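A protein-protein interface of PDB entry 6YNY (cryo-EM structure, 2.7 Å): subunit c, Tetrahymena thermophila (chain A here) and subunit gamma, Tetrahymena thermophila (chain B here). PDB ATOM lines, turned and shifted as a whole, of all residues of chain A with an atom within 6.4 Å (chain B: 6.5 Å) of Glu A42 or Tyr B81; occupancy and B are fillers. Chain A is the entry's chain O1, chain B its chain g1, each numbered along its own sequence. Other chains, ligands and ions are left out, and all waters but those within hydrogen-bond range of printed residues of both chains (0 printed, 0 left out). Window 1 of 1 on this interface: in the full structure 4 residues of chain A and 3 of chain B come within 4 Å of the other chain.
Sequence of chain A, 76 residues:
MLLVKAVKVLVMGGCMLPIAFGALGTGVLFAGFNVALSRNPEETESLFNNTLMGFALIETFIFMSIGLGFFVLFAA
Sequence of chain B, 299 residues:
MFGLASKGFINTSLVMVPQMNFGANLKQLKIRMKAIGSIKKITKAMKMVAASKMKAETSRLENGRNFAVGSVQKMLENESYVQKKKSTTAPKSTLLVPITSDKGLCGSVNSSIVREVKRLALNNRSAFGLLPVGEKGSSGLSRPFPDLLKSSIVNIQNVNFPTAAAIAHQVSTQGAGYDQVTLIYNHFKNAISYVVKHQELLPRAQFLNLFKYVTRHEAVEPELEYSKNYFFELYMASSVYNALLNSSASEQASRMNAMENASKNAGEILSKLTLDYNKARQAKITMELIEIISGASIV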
ATOM      1  N   LEU A  37       7.989 -37.924  -4.750  1.00  0.00           N
ATOM      2  CA  LEU A  37       6.972 -36.888  -4.884  1.00  0.00           C
ATOM      3  C   LEU A  37       6.654 -36.250  -3.538  1.00  0.00           C
ATOM      4  O   LEU A  37       6.514 -35.025  -3.444  1.00  0.00           O
ATOM      5  CB  LEU A  37       5.712 -37.478  -5.515  1.00  0.00           C
ATOM      6  CG  LEU A  37       4.553 -36.516  -5.757  1.00  0.00           C
ATOM      7  CD1 LEU A  37       4.993 -35.384  -6.660  1.00  0.00           C
ATOM      8  CD2 LEU A  37       3.380 -37.259  -6.367  1.00  0.00           C
ATOM      9  N   ASN A  40       9.142 -33.643  -2.483  1.00  0.00           N
ATOM     10  CA  ASN A  40       9.081 -32.385  -3.228  1.00  0.00           C
ATOM     11  C   ASN A  40       7.855 -32.405  -4.125  1.00  0.00           C
ATOM     12  O   ASN A  40       7.955 -32.588  -5.345  1.00  0.00           O
ATOM     13  CB  ASN A  40      10.354 -32.171  -4.047  1.00  0.00           C
ATOM     14  CG  ASN A  40      10.404 -30.806  -4.701  1.00  0.00           C
ATOM     15  OD1 ASN A  40       9.509 -29.982  -4.514  1.00  0.00           O
ATOM     16  ND2 ASN A  40      11.459 -30.556  -5.468  1.00  0.00           N
ATOM     17  N   PRO A  41       6.664 -32.210  -3.551  1.00  0.00           N
ATOM     18  CA  PRO A  41       5.436 -32.278  -4.355  1.00  0.00           C
ATOM     19  C   PRO A  41       5.180 -31.050  -5.210  1.00  0.00           C
ATOM     20  O   PRO A  41       4.292 -31.097  -6.074  1.00  0.00           O
ATOM     21  CB  PRO A  41       4.340 -32.445  -3.296  1.00  0.00           C
ATOM     22  CG  PRO A  41       4.888 -31.789  -2.088  1.00  0.00           C
ATOM     23  CD  PRO A  41       6.377 -31.999  -2.122  1.00  0.00           C
ATOM     24  N   GLU A  42       5.916 -29.956  -4.999  1.00  0.00           N
ATOM     25  CA  GLU A  42       5.664 -28.741  -5.766  1.00  0.00           C
ATOM     26  C   GLU A  42       5.883 -28.963  -7.255  1.00  0.00           C
ATOM     27  O   GLU A  42       5.212 -28.335  -8.082  1.00  0.00           O
ATOM     28  CB  GLU A  42       6.558 -27.608  -5.264  1.00  0.00           C
ATOM     29  CG  GLU A  42       6.322 -26.277  -5.966  1.00  0.00           C
ATOM     30  CD  GLU A  42       7.218 -25.174  -5.440  1.00  0.00           C
ATOM     31  OE1 GLU A  42       8.014 -25.441  -4.515  1.00  0.00           O
ATOM     32  OE2 GLU A  42       7.127 -24.038  -5.952  1.00  0.00           O
ATOM     33  N   GLU A  43       6.808 -29.847  -7.615  1.00  0.00           N
ATOM     34  CA  GLU A  43       7.153 -30.125  -9.005  1.00  0.00           C
ATOM     35  C   GLU A  43       6.642 -31.497  -9.438  1.00  0.00           C
ATOM     36  O   GLU A  43       7.317 -32.233 -10.159  1.00  0.00           O
ATOM     37  CB  GLU A  43       8.662 -30.011  -9.213  1.00  0.00           C
ATOM     38  CG  GLU A  43       9.492 -30.807  -8.223  1.00  0.00           C
ATOM     39  CD  GLU A  43      10.979 -30.675  -8.476  1.00  0.00           C
ATOM     40  OE1 GLU A  43      11.357 -30.111  -9.523  1.00  0.00           O
ATOM     41  OE2 GLU A  43      11.769 -31.132  -7.624  1.00  0.00           O
ATOM     42  N   THR A  44       5.436 -31.849  -8.988  1.00  0.00           N
ATOM     43  CA  THR A  44       4.838 -33.129  -9.355  1.00  0.00           C
ATOM     44  C   THR A  44       4.823 -33.323 -10.867  1.00  0.00           C
ATOM     45  O   THR A  44       5.048 -34.432 -11.362  1.00  0.00           O
ATOM     46  CB  THR A  44       3.417 -33.226  -8.792  1.00  0.00           C
ATOM     47  OG1 THR A  44       2.890 -34.536  -9.034  1.00  0.00           O
ATOM     48  CG2 THR A  44       2.502 -32.197  -9.436  1.00  0.00           C
ATOM     49  N   GLU A  45       4.553 -32.252 -11.617  1.00  0.00           N
ATOM     50  CA  GLU A  45       4.463 -32.369 -13.069  1.00  0.00           C
ATOM     51  C   GLU A  45       5.770 -32.872 -13.669  1.00  0.00           C
ATOM     52  O   GLU A  45       5.761 -33.703 -14.585  1.00  0.00           O
ATOM     53  CB  GLU A  45       4.067 -31.023 -13.683  1.00  0.00           C
ATOM     54  CG  GLU A  45       5.173 -29.966 -13.729  1.00  0.00           C
ATOM     55  CD  GLU A  45       5.649 -29.543 -12.353  1.00  0.00           C
ATOM     56  OE1 GLU A  45       4.982 -29.891 -11.357  1.00  0.00           O
ATOM     57  OE2 GLU A  45       6.693 -28.863 -12.268  1.00  0.00           O
ATOM     58  N   ASN B  78      12.000 -18.669   1.377  1.00  0.00           N
ATOM     59  CA  ASN B  78      12.504 -19.467   0.266  1.00  0.00           C
ATOM     60  C   ASN B  78      11.668 -20.719   0.041  1.00  0.00           C
ATOM     61  O   ASN B  78      11.657 -21.249  -1.076  1.00  0.00           O
ATOM     62  CB  ASN B  78      13.960 -19.860   0.516  1.00  0.00           C
ATOM     63  CG  ASN B  78      14.881 -18.661   0.597  1.00  0.00           C
ATOM     64  OD1 ASN B  78      14.621 -17.621  -0.008  1.00  0.00           O
ATOM     65  ND2 ASN B  78      15.967 -18.799   1.348  1.00  0.00           N
ATOM     66  N   GLU B  79      10.974 -21.200   1.069  1.00  0.00           N
ATOM     67  CA  GLU B  79      10.102 -22.363   0.939  1.00  0.00           C
ATOM     68  C   GLU B  79       8.882 -21.958   0.126  1.00  0.00           C
ATOM     69  O   GLU B  79       7.931 -21.379   0.656  1.00  0.00           O
ATOM     70  CB  GLU B  79       9.700 -22.888   2.312  1.00  0.00           C
ATOM     71  CG  GLU B  79      10.838 -23.528   3.086  1.00  0.00           C
ATOM     72  CD  GLU B  79      11.312 -24.824   2.466  1.00  0.00           C
ATOM     73  OE1 GLU B  79      10.565 -25.402   1.650  1.00  0.00           O
ATOM     74  OE2 GLU B  79      12.435 -25.262   2.789  1.00  0.00           O
ATOM     75  N   SER B  80       8.900 -22.264  -1.170  1.00  0.00           N
ATOM     76  CA  SER B  80       7.777 -21.898  -2.023  1.00  0.00           C
ATOM     77  C   SER B  80       6.538 -22.713  -1.677  1.00  0.00           C
ATOM     78  O   SER B  80       5.451 -22.156  -1.485  1.00  0.00           O
ATOM     79  CB  SER B  80       8.157 -22.086  -3.491  1.00  0.00           C
ATOM     80  OG  SER B  80       8.763 -23.350  -3.702  1.00  0.00           O
ATOM     81  N   TYR B  81       6.684 -24.037  -1.579  1.00  0.00           N
ATOM     82  CA  TYR B  81       5.534 -24.883  -1.278  1.00  0.00           C
ATOM     83  C   TYR B  81       4.868 -24.480   0.031  1.00  0.00           C
ATOM     84  O   TYR B  81       3.652 -24.641   0.184  1.00  0.00           O
ATOM     85  CB  TYR B  81       5.970 -26.348  -1.224  1.00  0.00           C
ATOM     86  CG  TYR B  81       4.842 -27.319  -0.960  1.00  0.00           C
ATOM     87  CD1 TYR B  81       3.989 -27.718  -1.981  1.00  0.00           C
ATOM     88  CD2 TYR B  81       4.634 -27.843   0.309  1.00  0.00           C
ATOM     89  CE1 TYR B  81       2.958 -28.606  -1.744  1.00  0.00           C
ATOM     90  CE2 TYR B  81       3.606 -28.731   0.555  1.00  0.00           C
ATOM     91  CZ  TYR B  81       2.771 -29.109  -0.474  1.00  0.00           C
ATOM     92  OH  TYR B  81       1.746 -29.993  -0.231  1.00  0.00           O
ATOM     93  N   VAL B  82       5.642 -23.956   0.981  1.00  0.00           N
ATOM     94  CA  VAL B  82       5.069 -23.519   2.250  1.00  0.00           C
ATOM     95  C   VAL B  82       4.161 -22.313   2.039  1.00  0.00           C
ATOM     96  O   VAL B  82       3.031 -22.270   2.542  1.00  0.00           O
ATOM     97  CB  VAL B  82       6.188 -23.211   3.261  1.00  0.00           C
ATOM     98  CG1 VAL B  82       5.620 -22.526   4.493  1.00  0.00           C
ATOM     99  CG2 VAL B  82       6.914 -24.486   3.647  1.00  0.00           C
ATOM    100  N   GLN B  83       4.643 -21.315   1.294  1.00  0.00           N
ATOM    101  CA  GLN B  83       3.840 -20.120   1.055  1.00  0.00           C
ATOM    102  C   GLN B  83       2.533 -20.460   0.351  1.00  0.00           C
ATOM    103  O   GLN B  83       1.497 -19.840   0.618  1.00  0.00           O
ATOM    104  CB  GLN B  83       4.643 -19.108   0.239  1.00  0.00           C
ATOM    105  CG  GLN B  83       5.612 -18.270   1.064  1.00  0.00           C
ATOM    106  CD  GLN B  83       6.575 -19.112   1.878  1.00  0.00           C
ATOM    107  OE1 GLN B  83       6.222 -19.630   2.937  1.00  0.00           O
ATOM    108  NE2 GLN B  83       7.800 -19.254   1.386  1.00  0.00           N
ATOM    109  N   LYS B  84       2.559 -21.443  -0.550  1.00  0.00           N
ATOM    110  CA  LYS B  84       1.333 -21.844  -1.231  1.00  0.00           C
ATOM    111  C   LYS B  84       0.288 -22.328  -0.234  1.00  0.00           C
ATOM    112  O   LYS B  84      -0.899 -22.004  -0.359  1.00  0.00           O
ATOM    113  CB  LYS B  84       1.632 -22.935  -2.260  1.00  0.00           C
ATOM    114  CG  LYS B  84       2.741 -22.594  -3.250  1.00  0.00           C
ATOM    115  CD  LYS B  84       2.451 -21.323  -4.036  1.00  0.00           C
ATOM    116  CE  LYS B  84       1.223 -21.475  -4.923  1.00  0.00           C
ATOM    117  NZ  LYS B  84       0.983 -20.269  -5.761  1.00  0.00           N
ATOM    118  N   LYS B  85       0.712 -23.102   0.762  1.00  0.00           N
ATOM    119  CA  LYS B  85      -0.179 -23.646   1.777  1.00  0.00           C
ATOM    120  C   LYS B  85      -0.123 -22.870   3.085  1.00  0.00           C
ATOM    121  O   LYS B  85      -0.738 -23.292   4.070  1.00  0.00           O
ATOM    122  CB  LYS B  85       0.160 -25.117   2.031  1.00  0.00           C
ATOM    123  CG  LYS B  85      -0.429 -26.080   1.008  1.00  0.00           C
ATOM    124  CD  LYS B  85      -0.023 -25.728  -0.413  1.00  0.00           C
ATOM    125  CE  LYS B  85      -0.496 -26.777  -1.402  1.00  0.00           C
ATOM    126  NZ  LYS B  85      -1.979 -26.898  -1.408  1.00  0.00           N
ATOM    127  N   LYS B  86       0.597 -21.752   3.121  1.00  0.00           N
ATOM    128  CA  LYS B  86       0.703 -20.976   4.348  1.00  0.00           C
ATOM    129  C   LYS B  86      -0.678 -20.516   4.796  1.00  0.00           C
ATOM    130  O   LYS B  86      -1.424 -19.903   4.027  1.00  0.00           O
ATOM    131  CB  LYS B  86       1.619 -19.772   4.126  1.00  0.00           C
ATOM    132  CG  LYS B  86       1.904 -18.958   5.380  1.00  0.00           C
ATOM    133  CD  LYS B  86       2.471 -17.587   5.046  1.00  0.00           C
ATOM    134  CE  LYS B  86       3.792 -17.675   4.295  1.00  0.00           C
ATOM    135  NZ  LYS B  86       4.830 -18.422   5.054  1.00  0.00           N
ATOM    136  N   TYR B 213       5.518 -28.283   6.896  1.00  0.00           N
ATOM    137  CA  TYR B 213       5.365 -28.283   5.447  1.00  0.00           C
ATOM    138  C   TYR B 213       6.678 -28.025   4.721  1.00  0.00           C
ATOM    139  O   TYR B 213       6.702 -28.067   3.487  1.00  0.00           O
ATOM    140  CB  TYR B 213       4.339 -27.231   5.015  1.00  0.00           C
ATOM    141  CG  TYR B 213       2.969 -27.392   5.635  1.00  0.00           C
ATOM    142  CD1 TYR B 213       2.081 -26.326   5.681  1.00  0.00           C
ATOM    143  CD2 TYR B 213       2.564 -28.604   6.179  1.00  0.00           C
ATOM    144  CE1 TYR B 213       0.830 -26.463   6.246  1.00  0.00           C
ATOM    145  CE2 TYR B 213       1.315 -28.749   6.746  1.00  0.00           C
ATOM    146  CZ  TYR B 213       0.454 -27.676   6.780  1.00  0.00           C
ATOM    147  OH  TYR B 213      -0.792 -27.821   7.345  1.00  0.00           O
ATOM    148  N   VAL B 214       7.761 -27.756   5.451  1.00  0.00           N
ATOM    149  CA  VAL B 214       9.045 -27.476   4.818  1.00  0.00           C
ATOM    150  C   VAL B 214       9.468 -28.676   3.987  1.00  0.00           C
ATOM    151  O   VAL B 214       9.588 -29.797   4.498  1.00  0.00           O
ATOM    152  CB  VAL B 214      10.101 -27.129   5.872  1.00  0.00           C
ATOM    153  CG1 VAL B 214      11.489 -27.146   5.253  1.00  0.00           C
ATOM    154  CG2 VAL B 214       9.810 -25.770   6.486  1.00  0.00           C
ATOM    155  N   THR B 215       9.693 -28.447   2.694  1.00  0.00           N
ATOM    156  CA  THR B 215      10.134 -29.493   1.783  1.00  0.00           C
ATOM    157  C   THR B 215      11.307 -29.091   0.902  1.00  0.00           C
ATOM    158  O   THR B 215      12.014 -29.981   0.415  1.00  0.00           O
ATOM    159  CB  THR B 215       8.974 -29.934   0.876  1.00  0.00           C
ATOM    160  OG1 THR B 215       9.417 -30.971  -0.007  1.00  0.00           O
ATOM    161  CG2 THR B 215       8.454 -28.759   0.058  1.00  0.00           C
ATOM    162  N   ARG B 216      11.541 -27.797   0.681  1.00  0.00           N
ATOM    163  CA  ARG B 216      12.652 -27.384  -0.171  1.00  0.00           C
ATOM    164  C   ARG B 216      13.992 -27.608   0.520  1.00  0.00           C
ATOM    165  O   ARG B 216      14.976 -27.982  -0.128  1.00  0.00           O
ATOM    166  CB  ARG B 216      12.485 -25.916  -0.561  1.00  0.00           C
ATOM    167  CG  ARG B 216      13.370 -25.464  -1.708  1.00  0.00           C
ATOM    168  CD  ARG B 216      13.354 -23.950  -1.848  1.00  0.00           C
ATOM    169  NE  ARG B 216      13.960 -23.504  -3.101  1.00  0.00           N
ATOM    170  CZ  ARG B 216      13.293 -23.307  -4.234  1.00  0.00           C
ATOM    171  NH1 ARG B 216      13.940 -22.902  -5.318  1.00  0.00           N
ATOM    172  NH2 ARG B 216      11.983 -23.513  -4.294  1.00  0.00           N
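OG of Ser B80 sits at hydrogen-bond distance from OE2 of Glu A42 (2.9 Å).
The backbone NH of Thr B215 is in hydrogen-bond range of the side-chain carboxylate of Glu B79. OG of Ser B80 sits at hydrogen-bond distance from NH2 of Arg B216 (3.3 Å).
Among the printed residues, merely in contact across the chains: Glu A42 with Tyr B81 (3.5 Å), Asn A40 with Thr B215 (3.5 Å), Pro A41 with Tyr B81 (3.7 Å) and Pro A41 with Thr B215 (3.8 Å).
Of the printed residues of chain B, Glu A42 touches Ser B80 and Tyr B81. Of chain A, only Pro A41 (3.7 Å) and Glu A42 (3.5 Å) come within 4 Å of Tyr B81. Printed residues of chain A within 4 Å of Thr B215: Asn A40 (3.5 Å) and Pro A41 (3.8 Å). Printed residues of chain B within 4 Å of Pro A41: Tyr B81 (3.7 Å) and Thr B215 (3.8 Å). Printed residues of chain B within 4 Å of Asn A40: Thr B215. Of the printed residues of chain A, Ser B80 touches Glu A42 (2.4 Å).
Of the 13 printed residues of chain B, 3 touch a printed residue of chain A. Along chain B the printed residues that touch a printed residue of chain A span positions 80 to 215. Hydrophobic or aromatic side chains of chain A that line the printed part of chain B: Pro A41. Among the printed residues, 5 pairs touch across the chains. Among the printed residues, no Asp or Glu carboxylate lies within 4 Å of a Lys or Arg side-chain nitrogen of the other chain.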
